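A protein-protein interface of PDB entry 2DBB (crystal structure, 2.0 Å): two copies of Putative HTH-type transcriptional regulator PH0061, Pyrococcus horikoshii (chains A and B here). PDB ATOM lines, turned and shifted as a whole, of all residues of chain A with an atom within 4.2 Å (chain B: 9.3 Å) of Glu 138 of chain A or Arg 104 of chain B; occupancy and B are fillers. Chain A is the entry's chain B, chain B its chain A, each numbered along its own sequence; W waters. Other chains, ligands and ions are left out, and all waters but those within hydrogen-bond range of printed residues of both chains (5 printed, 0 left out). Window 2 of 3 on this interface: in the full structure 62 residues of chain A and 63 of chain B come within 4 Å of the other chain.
OH of Tyr 105 of chain B lies within hydrogen-bond range of NH1 of Arg 104 of chain A (3.2 Å).
The side-chain hydroxyl of Tyr 105 of chain B lies within hydrogen-bond range of the side-chain hydroxyl of Tyr 105 of chain A, 3.4 Å away.
OE1 of Glu 138 of chain B lies within salt-bridge range of NE of Arg 104 of chain A, at 3.5 Å.
Among the printed residues, pairs that only touch across the chains: Ile 140 of chain A with Tyr 105 of chain B (3.6 Å), Glu 138 of chain A with Arg 104 of chain B (3.6 Å), Ile 140 of chain A with Arg 104 of chain B (3.6 Å), Ile 140 of chain A with Val 102 of chain B (3.6 Å), Tyr 105 of chain A with Leu 73 of chain B (3.7 Å), Ile 71 of chain A with Ile 108 of chain B (3.7 Å), Leu 73 of chain A with Tyr 105 of chain B (3.8 Å), Ile 140 of chain A with Ile 108 of chain B (3.8 Å), Ile 140 of chain A with Gly 101 of chain B (3.9 Å), Leu 73 of chain A with Leu 73 of chain B (3.96 Å) and Val 139 of chain A with Val 102 of chain B (3.96 Å).
Leu 73 of chain A touches its own counterpart, Leu 73 of chain B.
Leu 73 of chain A touches Tyr 105 of chain B, and with the chains exchanged Tyr 105 of chain A touches Leu 73 of chain B.
Arg 104 of chain A touches Tyr 105 of chain B, but with the chains exchanged Tyr 105 of chain A does not touch Arg 104 of chain B (4.8 Å).
Arg 104 of chain A touches Glu 138 of chain B, and with the chains exchanged Glu 138 of chain A touches Arg 104 of chain B.
5 positions are printed for both chains.
Of the 17 printed residues of chain B, 7 touch a printed residue of chain A.
Hydrophobic or aromatic side chains of chain A that line the printed part of chain B: Ile 71, Leu 73, Tyr 105 and Ile 140.
Among the printed residues, Asp or Glu carboxylates within 4 Å of a Lys or Arg side-chain nitrogen of the other chain: Arg 104 of chain A with Glu 138 of chain B (3.5 Å).
Water W3 lies within hydrogen-bond range of O of Val 139 of chain A (2.5 Å) and O of Val 102 of chain B (2.7 Å).
Water W1 lies within hydrogen-bond range of the guanidinium group (NH1) of Arg 104 of chain A, the side-chain hydroxyl (OH) of Tyr 105 of chain B, the guanidinium group (NH2) of Arg 104 of chain B and the side-chain carboxylate (OE1) of Glu 138 of chain B.
Water W4 bridges NE of Arg 104 of chain A (2.8 Å) and OE1 of Glu 138 of chain B (3.1 Å).
Water W2 lies within hydrogen-bond range of OE1 of Glu 138 of chain A (2.8 Å), N of Arg 104 of chain B (2.9 Å) and O of Val 139 of chain A (3.1 Å).
Water W5 bridges N of Arg 104 of chain A (2.9 Å) and OE2 of Glu 138 of chain B (3.0 Å).
N of Leu 73 of chain B is in hydrogen-bond range of O of Glu 138 of chain B.
The backbone NH of Gly 101 of chain B sits at hydrogen-bond distance from the backbone carbonyl oxygen of Asn 106 of chain B (2.7 Å).
The guanidinium group of Arg 104 of chain B lies close to the side-chain amide nitrogen of Asn 136 of chain B, 3.0 Å away.
The backbone carbonyl oxygen of Ile 71 of chain A lies within hydrogen-bond range of the backbone NH of Ile 140 of chain A, 2.7 Å away.
O of Glu 138 of chain A lies within hydrogen-bond range of N of Leu 73 of chain A, 2.8 Å away.
Of chain B, only Arg 104 (3.6 Å) comes within 4 Å of Glu 138 of chain A.
Of the printed residues of chain A, Arg 104 of chain B touches Glu 138 (3.6 Å) and Ile 140 (3.6 Å).
Val 137 of chain A touches none of the printed residues of chain B.
Printed residues of chain B within 4 Å of Arg 104 of chain A: Tyr 105 (3.2 Å) and Glu 138 (3.5 Å).
Printed residues of chain A within 4 Å of Val 102 of chain B: Val 139 and Ile 140.
Of the printed residues of chain B, Ile 71 of chain A touches Ile 108 (3.7 Å).
Of the printed residues of chain B, Tyr 105 of chain A touches Leu 73 and Tyr 105.
Val 137 of chain B touches none of the printed residues of chain A.
The nearest printed residue of chain A that does not touch Arg 104 of chain B is Arg 104 of chain A (4.01 Å).
The nearest printed residue of chain B that does not touch Arg 104 of chain A is Arg 104 of chain B (4.01 Å).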
ATOM      1  N   ILE A  71      -8.576  -9.029  32.173  1.00  0.00           N
ATOM      2  CA  ILE A  71      -9.301  -8.592  33.347  1.00  0.00           C
ATOM      3  C   ILE A  71     -10.468  -9.556  33.467  1.00  0.00           C
ATOM      4  O   ILE A  71     -11.166  -9.812  32.489  1.00  0.00           O
ATOM      5  CB  ILE A  71      -9.861  -7.159  33.192  1.00  0.00           C
ATOM      6  CG1 ILE A  71      -8.715  -6.148  33.036  1.00  0.00           C
ATOM      7  CG2 ILE A  71     -10.717  -6.811  34.390  1.00  0.00           C
ATOM      8  CD1 ILE A  71      -7.852  -5.981  34.271  1.00  0.00           C
ATOM      9  N   VAL A  72     -10.652 -10.109  34.659  1.00  0.00           N
ATOM     10  CA  VAL A  72     -11.752 -11.028  34.903  1.00  0.00           C
ATOM     11  C   VAL A  72     -12.748 -10.362  35.850  1.00  0.00           C
ATOM     12  O   VAL A  72     -12.414  -9.967  36.971  1.00  0.00           O
ATOM     13  CB  VAL A  72     -11.240 -12.356  35.493  1.00  0.00           C
ATOM     14  CG1 VAL A  72     -12.410 -13.306  35.756  1.00  0.00           C
ATOM     15  CG2 VAL A  72     -10.257 -12.989  34.522  1.00  0.00           C
ATOM     16  N   LEU A  73     -13.970 -10.213  35.365  1.00  0.00           N
ATOM     17  CA  LEU A  73     -15.044  -9.588  36.118  1.00  0.00           C
ATOM     18  C   LEU A  73     -15.932 -10.708  36.649  1.00  0.00           C
ATOM     19  O   LEU A  73     -16.473 -11.507  35.882  1.00  0.00           O
ATOM     20  CB  LEU A  73     -15.837  -8.665  35.189  1.00  0.00           C
ATOM     21  CG  LEU A  73     -14.965  -7.690  34.380  1.00  0.00           C
ATOM     22  CD1 LEU A  73     -15.795  -7.057  33.272  1.00  0.00           C
ATOM     23  CD2 LEU A  73     -14.390  -6.628  35.301  1.00  0.00           C
ATOM     24  N   ARG A 104     -21.964  -3.941  39.300  1.00  0.00           N
ATOM     25  CA  ARG A 104     -22.343  -5.107  38.508  1.00  0.00           C
ATOM     26  C   ARG A 104     -21.499  -6.352  38.781  1.00  0.00           C
ATOM     27  O   ARG A 104     -21.980  -7.473  38.624  1.00  0.00           O
ATOM     28  CB  ARG A 104     -22.316  -4.791  37.011  1.00  0.00           C
ATOM     29  CG  ARG A 104     -22.741  -5.993  36.168  1.00  0.00           C
ATOM     30  CD  ARG A 104     -22.816  -5.724  34.670  1.00  0.00           C
ATOM     31  NE  ARG A 104     -24.145  -5.287  34.256  1.00  0.00           N
ATOM     32  CZ  ARG A 104     -24.609  -5.390  33.014  1.00  0.00           C
ATOM     33  NH1 ARG A 104     -23.847  -5.918  32.062  1.00  0.00           N
ATOM     34  NH2 ARG A 104     -25.829  -4.966  32.721  1.00  0.00           N
ATOM     35  N   TYR A 105     -20.243  -6.159  39.172  1.00  0.00           N
ATOM     36  CA  TYR A 105     -19.353  -7.276  39.477  1.00  0.00           C
ATOM     37  C   TYR A 105     -18.744  -7.022  40.851  1.00  0.00           C
ATOM     38  O   TYR A 105     -18.265  -5.917  41.125  1.00  0.00           O
ATOM     39  CB  TYR A 105     -18.253  -7.371  38.420  1.00  0.00           C
ATOM     40  CG  TYR A 105     -18.793  -7.514  37.019  1.00  0.00           C
ATOM     41  CD1 TYR A 105     -19.247  -8.744  36.549  1.00  0.00           C
ATOM     42  CD2 TYR A 105     -18.883  -6.408  36.168  1.00  0.00           C
ATOM     43  CE1 TYR A 105     -19.774  -8.871  35.268  1.00  0.00           C
ATOM     44  CE2 TYR A 105     -19.413  -6.526  34.887  1.00  0.00           C
ATOM     45  CZ  TYR A 105     -19.856  -7.758  34.448  1.00  0.00           C
ATOM     46  OH  TYR A 105     -20.390  -7.887  33.189  1.00  0.00           O
ATOM     47  N   VAL A 137     -19.234 -14.495  34.822  1.00  0.00           N
ATOM     48  CA  VAL A 137     -17.800 -14.318  34.695  1.00  0.00           C
ATOM     49  C   VAL A 137     -17.523 -13.734  33.309  1.00  0.00           C
ATOM     50  O   VAL A 137     -17.903 -14.317  32.299  1.00  0.00           O
ATOM     51  CB  VAL A 137     -17.036 -15.651  34.821  1.00  0.00           C
ATOM     52  CG1 VAL A 137     -15.551 -15.419  34.573  1.00  0.00           C
ATOM     53  CG2 VAL A 137     -17.248 -16.243  36.208  1.00  0.00           C
ATOM     54  N   GLU A 138     -16.877 -12.577  33.268  1.00  0.00           N
ATOM     55  CA  GLU A 138     -16.543 -11.927  32.005  1.00  0.00           C
ATOM     56  C   GLU A 138     -15.034 -11.791  31.913  1.00  0.00           C
ATOM     57  O   GLU A 138     -14.405 -11.266  32.825  1.00  0.00           O
ATOM     58  CB  GLU A 138     -17.146 -10.524  31.933  1.00  0.00           C
ATOM     59  CG  GLU A 138     -18.648 -10.458  31.839  1.00  0.00           C
ATOM     60  CD  GLU A 138     -19.175 -11.047  30.550  1.00  0.00           C
ATOM     61  OE1 GLU A 138     -18.389 -11.191  29.581  1.00  0.00           O
ATOM     62  OE2 GLU A 138     -20.386 -11.353  30.508  1.00  0.00           O
ATOM     63  N   VAL A 139     -14.453 -12.277  30.824  1.00  0.00           N
ATOM     64  CA  VAL A 139     -13.018 -12.154  30.629  1.00  0.00           C
ATOM     65  C   VAL A 139     -12.769 -11.097  29.555  1.00  0.00           C
ATOM     66  O   VAL A 139     -13.296 -11.194  28.443  1.00  0.00           O
ATOM     67  CB  VAL A 139     -12.377 -13.472  30.151  1.00  0.00           C
ATOM     68  CG1 VAL A 139     -10.885 -13.259  29.904  1.00  0.00           C
ATOM     69  CG2 VAL A 139     -12.595 -14.572  31.190  1.00  0.00           C
ATOM     70  N   ILE A 140     -11.986 -10.078  29.898  1.00  0.00           N
ATOM     71  CA  ILE A 140     -11.653  -9.026  28.940  1.00  0.00           C
ATOM     72  C   ILE A 140     -10.172  -9.134  28.600  1.00  0.00           C
ATOM     73  O   ILE A 140      -9.322  -8.987  29.476  1.00  0.00           O
ATOM     74  CB  ILE A 140     -11.883  -7.607  29.515  1.00  0.00           C
ATOM     75  CG1 ILE A 140     -13.294  -7.481  30.100  1.00  0.00           C
ATOM     76  CG2 ILE A 140     -11.655  -6.569  28.418  1.00  0.00           C
ATOM     77  CD1 ILE A 140     -14.399  -7.703  29.092  1.00  0.00           C
ATOM     78  N   LEU B  73     -16.175   0.481  33.559  1.00  0.00           N
ATOM     79  CA  LEU B  73     -16.246  -0.421  32.417  1.00  0.00           C
ATOM     80  C   LEU B  73     -17.027   0.295  31.330  1.00  0.00           C
ATOM     81  O   LEU B  73     -18.150   0.745  31.557  1.00  0.00           O
ATOM     82  CB  LEU B  73     -16.958  -1.721  32.797  1.00  0.00           C
ATOM     83  CG  LEU B  73     -16.400  -2.387  34.061  1.00  0.00           C
ATOM     84  CD1 LEU B  73     -17.267  -3.575  34.440  1.00  0.00           C
ATOM     85  CD2 LEU B  73     -14.957  -2.811  33.821  1.00  0.00           C
ATOM     86  N   ILE B  74     -16.434   0.391  30.150  1.00  0.00           N
ATOM     87  CA  ILE B  74     -17.081   1.091  29.056  1.00  0.00           C
ATOM     88  C   ILE B  74     -17.196   0.255  27.796  1.00  0.00           C
ATOM     89  O   ILE B  74     -16.241  -0.390  27.373  1.00  0.00           O
ATOM     90  CB  ILE B  74     -16.303   2.389  28.698  1.00  0.00           C
ATOM     91  CG1 ILE B  74     -16.220   3.298  29.921  1.00  0.00           C
ATOM     92  CG2 ILE B  74     -16.982   3.111  27.517  1.00  0.00           C
ATOM     93  CD1 ILE B  74     -15.220   4.433  29.773  1.00  0.00           C
ATOM     94  N   LYS B  75     -18.379   0.274  27.200  1.00  0.00           N
ATOM     95  CA  LYS B  75     -18.604  -0.432  25.952  1.00  0.00           C
ATOM     96  C   LYS B  75     -19.023   0.629  24.929  1.00  0.00           C
ATOM     97  O   LYS B  75     -20.106   1.210  25.029  1.00  0.00           O
ATOM     98  CB  LYS B  75     -19.706  -1.472  26.110  1.00  0.00           C
ATOM     99  CG  LYS B  75     -19.961  -2.268  24.839  1.00  0.00           C
ATOM    100  CD  LYS B  75     -18.698  -2.978  24.395  1.00  0.00           C
ATOM    101  CE  LYS B  75     -18.408  -2.698  22.934  1.00  0.00           C
ATOM    102  NZ  LYS B  75     -19.582  -3.033  22.088  1.00  0.00           N
ATOM    103  N   SER B  76     -18.154   0.889  23.960  1.00  0.00           N
ATOM    104  CA  SER B  76     -18.420   1.884  22.916  1.00  0.00           C
ATOM    105  C   SER B  76     -19.496   1.363  21.980  1.00  0.00           C
ATOM    106  O   SER B  76     -19.699   0.145  21.873  1.00  0.00           O
ATOM    107  CB  SER B  76     -17.154   2.137  22.094  1.00  0.00           C
ATOM    108  OG  SER B  76     -16.045   2.396  22.926  1.00  0.00           O
ATOM    109  N   LYS B  77     -20.173   2.276  21.294  1.00  0.00           N
ATOM    110  CA  LYS B  77     -21.205   1.888  20.348  1.00  0.00           C
ATOM    111  C   LYS B  77     -20.515   1.371  19.088  1.00  0.00           C
ATOM    112  O   LYS B  77     -20.994   0.436  18.462  1.00  0.00           O
ATOM    113  CB  LYS B  77     -22.114   3.072  20.012  1.00  0.00           C
ATOM    114  CG  LYS B  77     -22.895   3.596  21.206  1.00  0.00           C
ATOM    115  CD  LYS B  77     -24.053   4.478  20.768  1.00  0.00           C
ATOM    116  CE  LYS B  77     -24.852   4.969  21.965  1.00  0.00           C
ATOM    117  NZ  LYS B  77     -25.978   5.851  21.543  1.00  0.00           N
ATOM    118  N   GLY B 101      -9.795  -3.060  25.476  1.00  0.00           N
ATOM    119  CA  GLY B 101      -9.981  -4.491  25.626  1.00  0.00           C
ATOM    120  C   GLY B 101     -10.908  -5.130  24.619  1.00  0.00           C
ATOM    121  O   GLY B 101     -11.583  -4.440  23.863  1.00  0.00           O
ATOM    122  N   VAL B 102     -10.934  -6.460  24.624  1.00  0.00           N
ATOM    123  CA  VAL B 102     -11.785  -7.233  23.732  1.00  0.00           C
ATOM    124  C   VAL B 102     -12.707  -8.111  24.577  1.00  0.00           C
ATOM    125  O   VAL B 102     -12.246  -8.949  25.356  1.00  0.00           O
ATOM    126  CB  VAL B 102     -10.956  -8.149  22.819  1.00  0.00           C
ATOM    127  CG1 VAL B 102     -11.864  -8.795  21.776  1.00  0.00           C
ATOM    128  CG2 VAL B 102      -9.843  -7.353  22.156  1.00  0.00           C
ATOM    129  N   GLY B 103     -14.008  -7.922  24.411  1.00  0.00           N
ATOM    130  CA  GLY B 103     -14.966  -8.694  25.177  1.00  0.00           C
ATOM    131  C   GLY B 103     -16.233  -7.892  25.375  1.00  0.00           C
ATOM    132  O   GLY B 103     -16.594  -7.093  24.516  1.00  0.00           O
ATOM    133  N   ARG B 104     -16.905  -8.096  26.504  1.00  0.00           N
ATOM    134  CA  ARG B 104     -18.142  -7.383  26.804  1.00  0.00           C
ATOM    135  C   ARG B 104     -17.924  -5.865  26.922  1.00  0.00           C
ATOM    136  O   ARG B 104     -18.838  -5.077  26.673  1.00  0.00           O
ATOM    137  CB  ARG B 104     -18.750  -7.924  28.101  1.00  0.00           C
ATOM    138  CG  ARG B 104     -20.072  -7.286  28.478  1.00  0.00           C
ATOM    139  CD  ARG B 104     -21.174  -7.691  27.518  1.00  0.00           C
ATOM    140  NE  ARG B 104     -22.448  -7.066  27.870  1.00  0.00           N
ATOM    141  CZ  ARG B 104     -22.701  -5.766  27.742  1.00  0.00           C
ATOM    142  NH1 ARG B 104     -21.767  -4.947  27.262  1.00  0.00           N
ATOM    143  NH2 ARG B 104     -23.881  -5.280  28.105  1.00  0.00           N
ATOM    144  N   TYR B 105     -16.722  -5.465  27.328  1.00  0.00           N
ATOM    145  CA  TYR B 105     -16.387  -4.048  27.449  1.00  0.00           C
ATOM    146  C   TYR B 105     -15.075  -3.840  26.697  1.00  0.00           C
ATOM    147  O   TYR B 105     -14.192  -4.700  26.738  1.00  0.00           O
ATOM    148  CB  TYR B 105     -16.217  -3.663  28.921  1.00  0.00           C
ATOM    149  CG  TYR B 105     -17.444  -3.946  29.757  1.00  0.00           C
ATOM    150  CD1 TYR B 105     -18.542  -3.087  29.730  1.00  0.00           C
ATOM    151  CD2 TYR B 105     -17.528  -5.100  30.539  1.00  0.00           C
ATOM    152  CE1 TYR B 105     -19.697  -3.368  30.458  1.00  0.00           C
ATOM    153  CE2 TYR B 105     -18.674  -5.392  31.266  1.00  0.00           C
ATOM    154  CZ  TYR B 105     -19.754  -4.524  31.220  1.00  0.00           C
ATOM    155  OH  TYR B 105     -20.895  -4.817  31.923  1.00  0.00           O
ATOM    156  N   ASN B 106     -14.940  -2.715  25.998  1.00  0.00           N
ATOM    157  CA  ASN B 106     -13.708  -2.479  25.262  1.00  0.00           C
ATOM    158  C   ASN B 106     -12.808  -1.436  25.902  1.00  0.00           C
ATOM    159  O   ASN B 106     -11.703  -1.187  25.429  1.00  0.00           O
ATOM    160  CB  ASN B 106     -14.003  -2.149  23.783  1.00  0.00           C
ATOM    161  CG  ASN B 106     -14.808  -0.878  23.596  1.00  0.00           C
ATOM    162  OD1 ASN B 106     -15.793  -0.627  24.293  1.00  0.00           O
ATOM    163  ND2 ASN B 106     -14.403  -0.075  22.619  1.00  0.00           N
ATOM    164  N   ILE B 107     -13.281  -0.819  26.983  1.00  0.00           N
ATOM    165  CA  ILE B 107     -12.454   0.143  27.702  1.00  0.00           C
ATOM    166  C   ILE B 107     -12.594  -0.051  29.200  1.00  0.00           C
ATOM    167  O   ILE B 107     -13.702  -0.058  29.737  1.00  0.00           O
ATOM    168  CB  ILE B 107     -12.824   1.602  27.437  1.00  0.00           C
ATOM    169  CG1 ILE B 107     -12.939   1.881  25.942  1.00  0.00           C
ATOM    170  CG2 ILE B 107     -11.737   2.484  28.030  1.00  0.00           C
ATOM    171  CD1 ILE B 107     -13.401   3.300  25.656  1.00  0.00           C
ATOM    172  N   ILE B 108     -11.463  -0.195  29.873  1.00  0.00           N
ATOM    173  CA  ILE B 108     -11.461  -0.360  31.308  1.00  0.00           C
ATOM    174  C   ILE B 108     -10.588   0.744  31.889  1.00  0.00           C
ATOM    175  O   ILE B 108      -9.446   0.953  31.462  1.00  0.00           O
ATOM    176  CB  ILE B 108     -10.945  -1.758  31.703  1.00  0.00           C
ATOM    177  CG1 ILE B 108     -11.880  -2.816  31.105  1.00  0.00           C
ATOM    178  CG2 ILE B 108     -10.912  -1.901  33.216  1.00  0.00           C
ATOM    179  CD1 ILE B 108     -11.536  -4.250  31.474  1.00  0.00           C
ATOM    180  N   GLU B 135     -22.362   2.908  24.782  1.00  0.00           N
ATOM    181  CA  GLU B 135     -23.449   1.932  24.789  1.00  0.00           C
ATOM    182  C   GLU B 135     -23.694   1.499  26.241  1.00  0.00           C
ATOM    183  O   GLU B 135     -24.836   1.438  26.704  1.00  0.00           O
ATOM    184  CB  GLU B 135     -23.066   0.722  23.932  1.00  0.00           C
ATOM    185  CG  GLU B 135     -24.138  -0.349  23.810  1.00  0.00           C
ATOM    186  CD  GLU B 135     -25.446   0.192  23.266  1.00  0.00           C
ATOM    187  OE1 GLU B 135     -25.410   1.113  22.419  1.00  0.00           O
ATOM    188  OE2 GLU B 135     -26.512  -0.311  23.678  1.00  0.00           O
ATOM    189  N   ASN B 136     -22.611   1.199  26.952  1.00  0.00           N
ATOM    190  CA  ASN B 136     -22.702   0.801  28.350  1.00  0.00           C
ATOM    191  C   ASN B 136     -21.574   1.412  29.163  1.00  0.00           C
ATOM    192  O   ASN B 136     -20.433   1.461  28.712  1.00  0.00           O
ATOM    193  CB  ASN B 136     -22.612  -0.724  28.511  1.00  0.00           C
ATOM    194  CG  ASN B 136     -23.705  -1.463  27.773  1.00  0.00           C
ATOM    195  OD1 ASN B 136     -24.887  -1.199  27.970  1.00  0.00           O
ATOM    196  ND2 ASN B 136     -23.311  -2.410  26.927  1.00  0.00           N
ATOM    197  N   VAL B 137     -21.905   1.883  30.359  1.00  0.00           N
ATOM    198  CA  VAL B 137     -20.918   2.437  31.275  1.00  0.00           C
ATOM    199  C   VAL B 137     -21.271   1.904  32.656  1.00  0.00           C
ATOM    200  O   VAL B 137     -22.383   2.111  33.139  1.00  0.00           O
ATOM    201  CB  VAL B 137     -20.941   3.977  31.329  1.00  0.00           C
ATOM    202  CG1 VAL B 137     -19.885   4.459  32.304  1.00  0.00           C
ATOM    203  CG2 VAL B 137     -20.682   4.561  29.954  1.00  0.00           C
ATOM    204  N   GLU B 138     -20.330   1.203  33.277  1.00  0.00           N
ATOM    205  CA  GLU B 138     -20.543   0.631  34.607  1.00  0.00           C
ATOM    206  C   GLU B 138     -19.480   1.163  35.544  1.00  0.00           C
ATOM    207  O   GLU B 138     -18.297   1.107  35.227  1.00  0.00           O
ATOM    208  CB  GLU B 138     -20.434  -0.899  34.562  1.00  0.00           C
ATOM    209  CG  GLU B 138     -21.513  -1.580  33.753  1.00  0.00           C
ATOM    210  CD  GLU B 138     -22.884  -1.442  34.388  1.00  0.00           C
ATOM    211  OE1 GLU B 138     -23.881  -1.799  33.728  1.00  0.00           O
ATOM    212  OE2 GLU B 138     -22.963  -0.983  35.551  1.00  0.00           O
HETATM  213  O   HOH W   1     -23.266  -3.527  30.883  1.00  0.00           O
HETATM  214  O   HOH W   2     -16.282 -10.680  27.764  1.00  0.00           O
HETATM  215  O   HOH W   3     -12.669 -11.540  26.024  1.00  0.00           O
HETATM  216  O   HOH W   4     -25.637  -3.381  35.656  1.00  0.00           O
HETATM  217  O   HOH W   5     -21.684  -1.231  38.268  1.00  0.00           O
